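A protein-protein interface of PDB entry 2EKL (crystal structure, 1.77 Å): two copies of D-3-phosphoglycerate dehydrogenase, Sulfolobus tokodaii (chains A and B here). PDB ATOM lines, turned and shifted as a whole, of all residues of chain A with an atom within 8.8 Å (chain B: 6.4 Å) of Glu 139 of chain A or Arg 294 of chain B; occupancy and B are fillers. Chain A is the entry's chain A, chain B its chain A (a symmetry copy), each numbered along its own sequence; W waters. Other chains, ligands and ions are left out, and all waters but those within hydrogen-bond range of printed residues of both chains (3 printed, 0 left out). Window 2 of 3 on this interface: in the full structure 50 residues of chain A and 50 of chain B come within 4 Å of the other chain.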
ATOM      1  N   MET A 113      13.252  -2.186  -2.095  1.00  0.00           N
ATOM      2  CA  MET A 113      13.520  -1.120  -1.131  1.00  0.00           C
ATOM      3  C   MET A 113      14.914  -0.527  -1.349  1.00  0.00           C
ATOM      4  O   MET A 113      15.083   0.693  -1.390  1.00  0.00           O
ATOM      5  CB  MET A 113      13.404  -1.660   0.298  1.00  0.00           C
ATOM      6  CG  MET A 113      13.779  -0.640   1.369  1.00  0.00           C
ATOM      7  SD  MET A 113      13.596  -1.289   3.053  1.00  0.00           S
ATOM      8  CE  MET A 113      14.951  -2.458   3.123  1.00  0.00           C
ATOM      9  N   ILE A 114      15.909  -1.392  -1.494  1.00  0.00           N
ATOM     10  CA  ILE A 114      17.277  -0.930  -1.693  1.00  0.00           C
ATOM     11  C   ILE A 114      17.448  -0.296  -3.071  1.00  0.00           C
ATOM     12  O   ILE A 114      18.109   0.731  -3.202  1.00  0.00           O
ATOM     13  CB  ILE A 114      18.280  -2.091  -1.522  1.00  0.00           C
ATOM     14  CG1 ILE A 114      18.191  -2.632  -0.091  1.00  0.00           C
ATOM     15  CG2 ILE A 114      19.699  -1.605  -1.799  1.00  0.00           C
ATOM     16  CD1 ILE A 114      18.937  -3.945   0.126  1.00  0.00           C
ATOM     17  N   ALA A 117      15.944   3.165  -2.822  1.00  0.00           N
ATOM     18  CA  ALA A 117      16.757   4.031  -1.985  1.00  0.00           C
ATOM     19  C   ALA A 117      18.059   4.445  -2.662  1.00  0.00           C
ATOM     20  O   ALA A 117      18.544   5.559  -2.457  1.00  0.00           O
ATOM     21  CB  ALA A 117      17.069   3.324  -0.664  1.00  0.00           C
ATOM     22  N   ARG A 118      18.606   3.568  -3.496  1.00  0.00           N
ATOM     23  CA  ARG A 118      19.890   3.845  -4.123  1.00  0.00           C
ATOM     24  C   ARG A 118      19.882   4.109  -5.621  1.00  0.00           C
ATOM     25  O   ARG A 118      20.947   4.188  -6.235  1.00  0.00           O
ATOM     26  CB  ARG A 118      20.841   2.688  -3.805  1.00  0.00           C
ATOM     27  CG  ARG A 118      21.046   2.510  -2.307  1.00  0.00           C
ATOM     28  CD  ARG A 118      21.856   3.673  -1.745  1.00  0.00           C
ATOM     29  NE  ARG A 118      23.280   3.523  -2.041  1.00  0.00           N
ATOM     30  CZ  ARG A 118      24.110   2.751  -1.343  1.00  0.00           C
ATOM     31  NH1 ARG A 118      23.662   2.056  -0.300  1.00  0.00           N
ATOM     32  NH2 ARG A 118      25.391   2.673  -1.687  1.00  0.00           N
ATOM     33  N   GLU A 136      23.856   9.464  -6.277  1.00  0.00           N
ATOM     34  CA  GLU A 136      23.673   9.421  -4.829  1.00  0.00           C
ATOM     35  C   GLU A 136      22.256   9.072  -4.383  1.00  0.00           C
ATOM     36  O   GLU A 136      21.277   9.590  -4.920  1.00  0.00           O
ATOM     37  CB  GLU A 136      24.083  10.760  -4.212  1.00  0.00           C
ATOM     38  CG  GLU A 136      24.035  10.783  -2.692  1.00  0.00           C
ATOM     39  CD  GLU A 136      24.329  12.155  -2.119  1.00  0.00           C
ATOM     40  OE1 GLU A 136      25.489  12.604  -2.209  1.00  0.00           O
ATOM     41  OE2 GLU A 136      23.395  12.786  -1.586  1.00  0.00           O
ATOM     42  N   GLY A 137      22.163   8.191  -3.391  1.00  0.00           N
ATOM     43  CA  GLY A 137      20.875   7.784  -2.856  1.00  0.00           C
ATOM     44  C   GLY A 137      20.783   7.986  -1.348  1.00  0.00           C
ATOM     45  O   GLY A 137      21.402   8.899  -0.786  1.00  0.00           O
ATOM     46  N   LEU A 138      20.015   7.122  -0.692  1.00  0.00           N
ATOM     47  CA  LEU A 138      19.812   7.196   0.752  1.00  0.00           C
ATOM     48  C   LEU A 138      20.219   5.919   1.480  1.00  0.00           C
ATOM     49  O   LEU A 138      20.006   4.813   0.980  1.00  0.00           O
ATOM     50  CB  LEU A 138      18.337   7.478   1.050  1.00  0.00           C
ATOM     51  CG  LEU A 138      17.752   8.788   0.511  1.00  0.00           C
ATOM     52  CD1 LEU A 138      16.264   8.851   0.823  1.00  0.00           C
ATOM     53  CD2 LEU A 138      18.480   9.968   1.140  1.00  0.00           C
ATOM     54  N   GLU A 139      20.790   6.084   2.670  1.00  0.00           N
ATOM     55  CA  GLU A 139      21.203   4.956   3.504  1.00  0.00           C
ATOM     56  C   GLU A 139      19.983   4.500   4.318  1.00  0.00           C
ATOM     57  O   GLU A 139      19.104   5.308   4.642  1.00  0.00           O
ATOM     58  CB  GLU A 139      22.347   5.389   4.426  1.00  0.00           C
ATOM     59  CG  GLU A 139      22.918   4.287   5.297  1.00  0.00           C
ATOM     60  CD  GLU A 139      24.154   4.740   6.044  1.00  0.00           C
ATOM     61  OE1 GLU A 139      25.262   4.642   5.470  1.00  0.00           O
ATOM     62  OE2 GLU A 139      24.018   5.211   7.199  1.00  0.00           O
ATOM     63  N   LEU A 140      19.924   3.217   4.659  1.00  0.00           N
ATOM     64  CA  LEU A 140      18.773   2.684   5.381  1.00  0.00           C
ATOM     65  C   LEU A 140      18.971   2.415   6.864  1.00  0.00           C
ATOM     66  O   LEU A 140      18.024   2.534   7.648  1.00  0.00           O
ATOM     67  CB  LEU A 140      18.290   1.404   4.690  1.00  0.00           C
ATOM     68  CG  LEU A 140      17.809   1.638   3.254  1.00  0.00           C
ATOM     69  CD1 LEU A 140      17.683   0.309   2.508  1.00  0.00           C
ATOM     70  CD2 LEU A 140      16.478   2.373   3.285  1.00  0.00           C
ATOM     71  N   ALA A 141      20.189   2.046   7.241  1.00  0.00           N
ATOM     72  CA  ALA A 141      20.500   1.749   8.633  1.00  0.00           C
ATOM     73  C   ALA A 141      20.114   2.912   9.537  1.00  0.00           C
ATOM     74  O   ALA A 141      20.308   4.074   9.181  1.00  0.00           O
ATOM     75  CB  ALA A 141      21.990   1.445   8.778  1.00  0.00           C
ATOM     76  N   GLY A 142      19.557   2.589  10.702  1.00  0.00           N
ATOM     77  CA  GLY A 142      19.165   3.613  11.656  1.00  0.00           C
ATOM     78  C   GLY A 142      17.817   4.250  11.389  1.00  0.00           C
ATOM     79  O   GLY A 142      17.249   4.910  12.263  1.00  0.00           O
ATOM     80  N   LYS A 143      17.295   4.062  10.184  1.00  0.00           N
ATOM     81  CA  LYS A 143      16.004   4.635   9.852  1.00  0.00           C
ATOM     82  C   LYS A 143      14.874   3.715  10.286  1.00  0.00           C
ATOM     83  O   LYS A 143      15.102   2.566  10.673  1.00  0.00           O
ATOM     84  CB  LYS A 143      15.939   4.942   8.357  1.00  0.00           C
ATOM     85  CG  LYS A 143      16.910   6.055   7.987  1.00  0.00           C
ATOM     86  CD  LYS A 143      16.845   6.433   6.531  1.00  0.00           C
ATOM     87  CE  LYS A 143      17.880   7.499   6.223  1.00  0.00           C
ATOM     88  NZ  LYS A 143      17.960   7.763   4.769  1.00  0.00           N
ATOM     89  N   THR A 144      13.654   4.229  10.231  1.00  0.00           N
ATOM     90  CA  THR A 144      12.483   3.477  10.650  1.00  0.00           C
ATOM     91  C   THR A 144      11.663   2.952   9.482  1.00  0.00           C
ATOM     92  O   THR A 144      11.346   3.698   8.555  1.00  0.00           O
ATOM     93  CB  THR A 144      11.566   4.359  11.518  1.00  0.00           C
ATOM     94  OG1 THR A 144      12.283   4.784  12.683  1.00  0.00           O
ATOM     95  CG2 THR A 144      10.319   3.593  11.945  1.00  0.00           C
ATOM     96  N   MET A 164      19.112  -5.204   9.302  1.00  0.00           N
ATOM     97  CA  MET A 164      19.769  -4.152   8.534  1.00  0.00           C
ATOM     98  C   MET A 164      19.938  -2.905   9.406  1.00  0.00           C
ATOM     99  O   MET A 164      20.370  -1.858   8.932  1.00  0.00           O
ATOM    100  CB  MET A 164      18.940  -3.810   7.289  1.00  0.00           C
ATOM    101  CG  MET A 164      18.859  -4.951   6.276  1.00  0.00           C
ATOM    102  SD  MET A 164      17.768  -4.554   4.878  1.00  0.00           S
ATOM    103  CE  MET A 164      18.633  -3.179   4.141  1.00  0.00           C
ATOM    104  N   GLY A 165      19.586  -3.025  10.684  1.00  0.00           N
ATOM    105  CA  GLY A 165      19.731  -1.894  11.587  1.00  0.00           C
ATOM    106  C   GLY A 165      18.608  -0.873  11.540  1.00  0.00           C
ATOM    107  O   GLY A 165      18.763   0.249  12.032  1.00  0.00           O
ATOM    108  N   MET A 166      17.479  -1.245  10.946  1.00  0.00           N
ATOM    109  CA  MET A 166      16.337  -0.346  10.873  1.00  0.00           C
ATOM    110  C   MET A 166      15.426  -0.579  12.074  1.00  0.00           C
ATOM    111  O   MET A 166      15.381  -1.681  12.630  1.00  0.00           O
ATOM    112  CB  MET A 166      15.536  -0.585   9.586  1.00  0.00           C
ATOM    113  CG  MET A 166      16.349  -0.481   8.307  1.00  0.00           C
ATOM    114  SD  MET A 166      15.307  -0.542   6.821  1.00  0.00           S
ATOM    115  CE  MET A 166      14.709   1.156   6.818  1.00  0.00           C
ATOM    116  N   ASP A 198      10.344   6.113   7.676  1.00  0.00           N
ATOM    117  CA  ASP A 198      11.143   6.669   6.590  1.00  0.00           C
ATOM    118  C   ASP A 198      10.888   5.790   5.370  1.00  0.00           C
ATOM    119  O   ASP A 198      10.989   6.235   4.228  1.00  0.00           O
ATOM    120  CB  ASP A 198      12.620   6.662   6.980  1.00  0.00           C
ATOM    121  CG  ASP A 198      12.883   7.472   8.238  1.00  0.00           C
ATOM    122  OD1 ASP A 198      12.680   8.703   8.203  1.00  0.00           O
ATOM    123  OD2 ASP A 198      13.273   6.877   9.266  1.00  0.00           O
ATOM    124  N   VAL A 199      10.546   4.532   5.637  1.00  0.00           N
ATOM    125  CA  VAL A 199      10.228   3.566   4.593  1.00  0.00           C
ATOM    126  C   VAL A 199       8.935   2.878   5.007  1.00  0.00           C
ATOM    127  O   VAL A 199       8.762   2.517   6.173  1.00  0.00           O
ATOM    128  CB  VAL A 199      11.321   2.478   4.449  1.00  0.00           C
ATOM    129  CG1 VAL A 199      10.909   1.459   3.381  1.00  0.00           C
ATOM    130  CG2 VAL A 199      12.657   3.115   4.079  1.00  0.00           C
ATOM    131  N   ILE A 227       9.986   6.556   1.451  1.00  0.00           N
ATOM    132  CA  ILE A 227      10.162   5.573   0.388  1.00  0.00           C
ATOM    133  C   ILE A 227       9.041   4.569   0.623  1.00  0.00           C
ATOM    134  O   ILE A 227       8.880   4.055   1.734  1.00  0.00           O
ATOM    135  CB  ILE A 227      11.521   4.838   0.484  1.00  0.00           C
ATOM    136  CG1 ILE A 227      12.661   5.799   0.155  1.00  0.00           C
ATOM    137  CG2 ILE A 227      11.541   3.650  -0.480  1.00  0.00           C
ATOM    138  CD1 ILE A 227      14.038   5.204   0.366  1.00  0.00           C
ATOM    139  N   TYR A 252       9.973  10.200  -1.989  1.00  0.00           N
ATOM    140  CA  TYR A 252      11.296  10.052  -2.581  1.00  0.00           C
ATOM    141  C   TYR A 252      11.241   9.017  -3.698  1.00  0.00           C
ATOM    142  O   TYR A 252      11.852   9.188  -4.760  1.00  0.00           O
ATOM    143  CB  TYR A 252      12.299   9.602  -1.513  1.00  0.00           C
ATOM    144  CG  TYR A 252      13.719   9.481  -2.011  1.00  0.00           C
ATOM    145  CD1 TYR A 252      14.521  10.612  -2.174  1.00  0.00           C
ATOM    146  CD2 TYR A 252      14.264   8.236  -2.324  1.00  0.00           C
ATOM    147  CE1 TYR A 252      15.833  10.504  -2.634  1.00  0.00           C
ATOM    148  CE2 TYR A 252      15.576   8.118  -2.789  1.00  0.00           C
ATOM    149  CZ  TYR A 252      16.353   9.256  -2.938  1.00  0.00           C
ATOM    150  OH  TYR A 252      17.652   9.152  -3.384  1.00  0.00           O
ATOM    151  N   ALA B  97      38.554   9.165   6.486  1.00  0.00           N
ATOM    152  CA  ALA B  97      37.343   8.654   7.130  1.00  0.00           C
ATOM    153  C   ALA B  97      37.138   7.148   6.981  1.00  0.00           C
ATOM    154  O   ALA B  97      36.185   6.704   6.338  1.00  0.00           O
ATOM    155  CB  ALA B  97      36.121   9.400   6.587  1.00  0.00           C
ATOM    156  N   GLY B  99      35.940   3.458   7.326  1.00  0.00           N
ATOM    157  CA  GLY B  99      34.695   2.852   7.768  1.00  0.00           C
ATOM    158  C   GLY B  99      33.464   3.740   7.667  1.00  0.00           C
ATOM    159  O   GLY B  99      32.362   3.312   7.998  1.00  0.00           O
ATOM    160  N   ALA B 100      33.644   4.968   7.191  1.00  0.00           N
ATOM    161  CA  ALA B 100      32.547   5.926   7.075  1.00  0.00           C
ATOM    162  C   ALA B 100      31.346   5.509   6.220  1.00  0.00           C
ATOM    163  O   ALA B 100      30.242   6.018   6.417  1.00  0.00           O
ATOM    164  CB  ALA B 100      33.086   7.252   6.565  1.00  0.00           C
ATOM    165  N   SER B 101      31.545   4.589   5.284  1.00  0.00           N
ATOM    166  CA  SER B 101      30.447   4.188   4.410  1.00  0.00           C
ATOM    167  C   SER B 101      29.962   2.752   4.589  1.00  0.00           C
ATOM    168  O   SER B 101      29.163   2.264   3.787  1.00  0.00           O
ATOM    169  CB  SER B 101      30.856   4.388   2.950  1.00  0.00           C
ATOM    170  OG  SER B 101      31.819   3.428   2.556  1.00  0.00           O
ATOM    171  N   THR B 102      30.426   2.087   5.641  1.00  0.00           N
ATOM    172  CA  THR B 102      30.059   0.694   5.889  1.00  0.00           C
ATOM    173  C   THR B 102      28.612   0.296   5.597  1.00  0.00           C
ATOM    174  O   THR B 102      28.369  -0.557   4.743  1.00  0.00           O
ATOM    175  CB  THR B 102      30.393   0.278   7.341  1.00  0.00           C
ATOM    176  OG1 THR B 102      31.798   0.444   7.574  1.00  0.00           O
ATOM    177  CG2 THR B 102      30.019  -1.182   7.578  1.00  0.00           C
ATOM    178  N   ASP B 103      27.648   0.900   6.288  1.00  0.00           N
ATOM    179  CA  ASP B 103      26.251   0.513   6.075  1.00  0.00           C
ATOM    180  C   ASP B 103      25.745   0.741   4.656  1.00  0.00           C
ATOM    181  O   ASP B 103      24.919  -0.026   4.158  1.00  0.00           O
ATOM    182  CB  ASP B 103      25.323   1.213   7.079  1.00  0.00           C
ATOM    183  CG  ASP B 103      25.509   0.705   8.504  1.00  0.00           C
ATOM    184  OD1 ASP B 103      25.874  -0.480   8.685  1.00  0.00           O
ATOM    185  OD2 ASP B 103      25.272   1.489   9.450  1.00  0.00           O
ATOM    186  N   SER B 104      26.224   1.790   4.001  1.00  0.00           N
ATOM    187  CA  SER B 104      25.792   2.046   2.632  1.00  0.00           C
ATOM    188  C   SER B 104      26.338   0.968   1.695  1.00  0.00           C
ATOM    189  O   SER B 104      25.650   0.532   0.771  1.00  0.00           O
ATOM    190  CB  SER B 104      26.245   3.435   2.183  1.00  0.00           C
ATOM    191  OG  SER B 104      25.453   4.429   2.820  1.00  0.00           O
ATOM    192  N   ALA B 105      27.567   0.527   1.942  1.00  0.00           N
ATOM    193  CA  ALA B 105      28.173  -0.514   1.110  1.00  0.00           C
ATOM    194  C   ALA B 105      27.482  -1.851   1.378  1.00  0.00           C
ATOM    195  O   ALA B 105      27.251  -2.639   0.457  1.00  0.00           O
ATOM    196  CB  ALA B 105      29.680  -0.616   1.397  1.00  0.00           C
ATOM    197  N   GLU B 107      24.372  -2.330   2.356  1.00  0.00           N
ATOM    198  CA  GLU B 107      23.058  -2.299   1.742  1.00  0.00           C
ATOM    199  C   GLU B 107      23.124  -2.513   0.236  1.00  0.00           C
ATOM    200  O   GLU B 107      22.319  -3.259  -0.322  1.00  0.00           O
ATOM    201  CB  GLU B 107      22.361  -0.979   2.096  1.00  0.00           C
ATOM    202  CG  GLU B 107      21.892  -0.954   3.556  1.00  0.00           C
ATOM    203  CD  GLU B 107      21.780   0.445   4.136  1.00  0.00           C
ATOM    204  OE1 GLU B 107      21.582   1.409   3.367  1.00  0.00           O
ATOM    205  OE2 GLU B 107      21.873   0.575   5.376  1.00  0.00           O
ATOM    206  N   THR B 288      25.697   7.802  -0.651  1.00  0.00           N
ATOM    207  CA  THR B 288      24.420   8.102  -0.011  1.00  0.00           C
ATOM    208  C   THR B 288      24.634   9.428   0.704  1.00  0.00           C
ATOM    209  O   THR B 288      25.765   9.785   1.038  1.00  0.00           O
ATOM    210  CB  THR B 288      23.989   7.044   1.030  1.00  0.00           C
ATOM    211  OG1 THR B 288      24.968   6.957   2.073  1.00  0.00           O
ATOM    212  CG2 THR B 288      23.806   5.686   0.368  1.00  0.00           C
ATOM    213  N   LYS B 289      23.555  10.166   0.926  1.00  0.00           N
ATOM    214  CA  LYS B 289      23.644  11.448   1.612  1.00  0.00           C
ATOM    215  C   LYS B 289      24.276  11.254   2.990  1.00  0.00           C
ATOM    216  O   LYS B 289      25.168  12.012   3.398  1.00  0.00           O
ATOM    217  CB  LYS B 289      22.242  12.049   1.750  1.00  0.00           C
ATOM    218  CG  LYS B 289      22.170  13.313   2.594  1.00  0.00           C
ATOM    219  CD  LYS B 289      20.753  13.883   2.618  1.00  0.00           C
ATOM    220  CE  LYS B 289      19.726  12.873   3.127  1.00  0.00           C
ATOM    221  NZ  LYS B 289      19.955  12.473   4.547  1.00  0.00           N
ATOM    222  N   GLU B 290      23.823  10.221   3.693  1.00  0.00           N
ATOM    223  CA  GLU B 290      24.322   9.928   5.033  1.00  0.00           C
ATOM    224  C   GLU B 290      25.803   9.556   5.072  1.00  0.00           C
ATOM    225  O   GLU B 290      26.553  10.074   5.905  1.00  0.00           O
ATOM    226  CB  GLU B 290      23.489   8.807   5.673  1.00  0.00           C
ATOM    227  CG  GLU B 290      22.027   9.162   5.957  1.00  0.00           C
ATOM    228  CD  GLU B 290      21.136   9.139   4.719  1.00  0.00           C
ATOM    229  OE1 GLU B 290      21.596   8.701   3.642  1.00  0.00           O
ATOM    230  OE2 GLU B 290      19.959   9.548   4.833  1.00  0.00           O
ATOM    231  N   ALA B 291      26.229   8.656   4.186  1.00  0.00           N
ATOM    232  CA  ALA B 291      27.628   8.241   4.155  1.00  0.00           C
ATOM    233  C   ALA B 291      28.551   9.393   3.778  1.00  0.00           C
ATOM    234  O   ALA B 291      29.610   9.576   4.381  1.00  0.00           O
ATOM    235  CB  ALA B 291      27.818   7.081   3.178  1.00  0.00           C
ATOM    236  N   GLN B 292      28.147  10.171   2.781  1.00  0.00           N
ATOM    237  CA  GLN B 292      28.952  11.298   2.338  1.00  0.00           C
ATOM    238  C   GLN B 292      29.076  12.357   3.431  1.00  0.00           C
ATOM    239  O   GLN B 292      30.111  13.014   3.543  1.00  0.00           O
ATOM    240  CB  GLN B 292      28.357  11.909   1.068  1.00  0.00           C
ATOM    241  CG  GLN B 292      28.592  11.076  -0.192  1.00  0.00           C
ATOM    242  CD  GLN B 292      30.053  10.707  -0.389  1.00  0.00           C
ATOM    243  OE1 GLN B 292      30.466   9.578  -0.111  1.00  0.00           O
ATOM    244  NE2 GLN B 292      30.846  11.662  -0.856  1.00  0.00           N
ATOM    245  N   LYS B 293      28.027  12.522   4.234  1.00  0.00           N
ATOM    246  CA  LYS B 293      28.076  13.491   5.325  1.00  0.00           C
ATOM    247  C   LYS B 293      29.039  12.974   6.391  1.00  0.00           C
ATOM    248  O   LYS B 293      29.801  13.744   6.984  1.00  0.00           O
ATOM    249  CB  LYS B 293      26.691  13.698   5.946  1.00  0.00           C
ATOM    250  CG  LYS B 293      26.706  14.636   7.152  1.00  0.00           C
ATOM    251  CD  LYS B 293      25.350  14.708   7.837  1.00  0.00           C
ATOM    252  CE  LYS B 293      25.414  15.564   9.094  1.00  0.00           C
ATOM    253  NZ  LYS B 293      24.128  15.561   9.840  1.00  0.00           N
ATOM    254  N   ARG B 294      29.011  11.668   6.642  1.00  0.00           N
ATOM    255  CA  ARG B 294      29.912  11.098   7.637  1.00  0.00           C
ATOM    256  C   ARG B 294      31.364  11.224   7.182  1.00  0.00           C
ATOM    257  O   ARG B 294      32.256  11.452   8.002  1.00  0.00           O
ATOM    258  CB  ARG B 294      29.574   9.630   7.914  1.00  0.00           C
ATOM    259  CG  ARG B 294      28.298   9.435   8.724  1.00  0.00           C
ATOM    260  CD  ARG B 294      28.298   8.073   9.393  1.00  0.00           C
ATOM    261  NE  ARG B 294      28.324   7.007   8.404  1.00  0.00           N
ATOM    262  CZ  ARG B 294      27.253   6.563   7.756  1.00  0.00           C
ATOM    263  NH1 ARG B 294      26.057   7.091   8.001  1.00  0.00           N
ATOM    264  NH2 ARG B 294      27.384   5.601   6.852  1.00  0.00           N
ATOM    265  N   VAL B 295      31.605  11.073   5.882  1.00  0.00           N
ATOM    266  CA  VAL B 295      32.960  11.200   5.357  1.00  0.00           C
ATOM    267  C   VAL B 295      33.482  12.600   5.666  1.00  0.00           C
ATOM    268  O   VAL B 295      34.601  12.763   6.151  1.00  0.00           O
ATOM    269  CB  VAL B 295      33.006  10.960   3.828  1.00  0.00           C
ATOM    270  CG1 VAL B 295      34.363  11.372   3.271  1.00  0.00           C
ATOM    271  CG2 VAL B 295      32.760   9.484   3.529  1.00  0.00           C
ATOM    272  N   ALA B 296      32.659  13.607   5.401  1.00  0.00           N
ATOM    273  CA  ALA B 296      33.047  14.990   5.658  1.00  0.00           C
ATOM    274  C   ALA B 296      33.263  15.249   7.148  1.00  0.00           C
ATOM    275  O   ALA B 296      34.278  15.831   7.539  1.00  0.00           O
ATOM    276  CB  ALA B 296      31.986  15.944   5.109  1.00  0.00           C
ATOM    277  N   GLU B 297      32.314  14.815   7.975  1.00  0.00           N
ATOM    278  CA  GLU B 297      32.405  15.016   9.422  1.00  0.00           C
ATOM    279  C   GLU B 297      33.589  14.298  10.054  1.00  0.00           C
ATOM    280  O   GLU B 297      34.289  14.860  10.897  1.00  0.00           O
ATOM    281  CB  GLU B 297      31.125  14.546  10.113  1.00  0.00           C
ATOM    282  CG  GLU B 297      29.860  15.219   9.613  1.00  0.00           C
ATOM    283  CD  GLU B 297      28.653  14.868  10.458  1.00  0.00           C
ATOM    284  OE1 GLU B 297      28.491  13.678  10.800  1.00  0.00           O
ATOM    285  OE2 GLU B 297      27.862  15.780  10.774  1.00  0.00           O
ATOM    286  N   MET B 298      33.801  13.049   9.656  1.00  0.00           N
ATOM    287  CA  MET B 298      34.902  12.268  10.196  1.00  0.00           C
ATOM    288  C   MET B 298      36.249  12.830   9.771  1.00  0.00           C
ATOM    289  O   MET B 298      37.176  12.906  10.576  1.00  0.00           O
ATOM    290  CB  MET B 298      34.787  10.814   9.747  1.00  0.00           C
ATOM    291  CG  MET B 298      33.640  10.070  10.389  1.00  0.00           C
ATOM    292  SD  MET B 298      33.665   8.333   9.933  1.00  0.00           S
ATOM    293  CE  MET B 298      35.342   7.903  10.446  1.00  0.00           C
ATOM    294  N   THR B 299      36.362  13.217   8.505  1.00  0.00           N
ATOM    295  CA  THR B 299      37.614  13.770   8.016  1.00  0.00           C
ATOM    296  C   THR B 299      37.886  15.075   8.758  1.00  0.00           C
ATOM    297  O   THR B 299      39.021  15.361   9.135  1.00  0.00           O
ATOM    298  CB  THR B 299      37.560  14.023   6.495  1.00  0.00           C
ATOM    299  OG1 THR B 299      37.342  12.780   5.812  1.00  0.00           O
ATOM    300  CG2 THR B 299      38.873  14.633   6.004  1.00  0.00           C
HETATM  301  O   HOH W   1      20.970   2.106   0.921  1.00  0.00           O
HETATM  302  O   HOH W   2      25.299   4.135   9.289  1.00  0.00           O
HETATM  303  O   HOH W   3      22.033  -1.779   6.794  1.00  0.00           O
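No position is printed for both chains. Of the 21 pairs that touch across the chains among the printed residues, none has its exchanged pair printed and touching as well.
The side-chain hydroxyl of Thr 288 of chain B is in hydrogen-bond range of the side-chain hydroxyl of Ser 104 of chain B, at 2.7 Å. OE2 of Glu 290 of chain B lies within salt-bridge range of NZ of Lys 289 of chain B (2.9 Å).
Water W1 lies within hydrogen-bond range of the side-chain carboxylate of Glu 107 of chain B (2.6 Å), the backbone carbonyl oxygen of Leu 138 of chain A (2.9 Å) and the guanidinium group of Arg 118 of chain A (3.0 Å).
Of the 20 printed residues of chain A, 10 touch a printed residue of chain B. Hydrophobic or aromatic side chains of chain A within 4 Å of the printed part of chain B: Ile 114, Leu 138, Leu 140, Ala 141 and Met 164. Printed residues of chain B that touch a printed residue of chain A: Asp 103, Ser 104, Glu 107, Thr 288, Lys 289, Glu 290 and Arg 294.
Among the printed residues, pairs that only touch across the chains: Gly 137 of chain A with Thr 288 of chain B (3.2 Å), Arg 118 of chain A with Thr 288 of chain B (3.3 Å), Ala 141 of chain A with Asp 103 of chain B (3.4 Å), Ile 114 of chain A with Glu 107 of chain B (3.4 Å), Glu 136 of chain A with Lys 289 of chain B (3.5 Å), Glu 139 of chain A with Glu 107 of chain B (3.6 Å), Glu 136 of chain A with Thr 288 of chain B (3.7 Å), Leu 138 of chain A with Glu 290 of chain B (3.7 Å), Glu 139 of chain A with Thr 288 of chain B (3.7 Å), Leu 138 of chain A with Lys 289 of chain B (3.7 Å), Leu 138 of chain A with Thr 288 of chain B (3.8 Å), Glu 139 of chain A with Asp 103 of chain B (3.8 Å) and Met 164 of chain A with Glu 107 of chain B (3.99 Å).
The guanidinium group (NH1) of Arg 118 of chain A sits at hydrogen-bond distance from the backbone carbonyl oxygen (O) of Ser 104 of chain B, at 2.7 Å. The backbone carbonyl oxygen (O) of Gly 137 of chain A lies within hydrogen-bond range of the backbone NH (N) of Lys 289 of chain B, 3.0 Å away. The side-chain hydroxyl of Ser 104 of chain B is in hydrogen-bond range of the side-chain carboxylate of Glu 139 of chain A (2.7 Å). The backbone NH (N) of Glu 139 of chain A sits at hydrogen-bond distance from the side-chain carboxylate (OE1) of Glu 290 of chain B (2.9 Å). The side-chain carboxylate (OE1) of Glu 139 of chain A is in salt-bridge range of the guanidinium group (NH2) of Arg 294 of chain B (2.7 Å). N of Leu 140 of chain A is in hydrogen-bond range of OE1 of Glu 107 of chain B (2.8 Å). The side-chain carboxylate (OE2) of Glu 107 of chain B sits at hydrogen-bond distance from the backbone NH (N) of Ala 141 of chain A, at 2.9 Å. The side-chain amino group of Lys 143 of chain A is in salt-bridge range of the side-chain carboxylate of Glu 290 of chain B (2.7 Å).
Of the printed residues of chain B, Arg 118 of chain A touches Ser 104 and Thr 288. Of chain B, only Asp 103 (3.8 Å), Ser 104 (2.7 Å), Glu 107 (3.6 Å), Thr 288 (3.7 Å), Glu 290 (2.9 Å) and Arg 294 (2.7 Å) come within 4 Å of Glu 139 of chain A. Of the printed residues of chain A, Asp 103 of chain B touches Glu 139 (3.8 Å) and Ala 141 (3.4 Å). Of chain A, only Glu 139 comes within 4 Å of Arg 294 of chain B. The nearest residue of chain B that does not touch Glu 139 of chain A is Ala 291 of chain B (4.2 Å). The nearest residue of chain A that does not touch Arg 294 of chain B is Ala 141 of chain A (6.6 Å).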
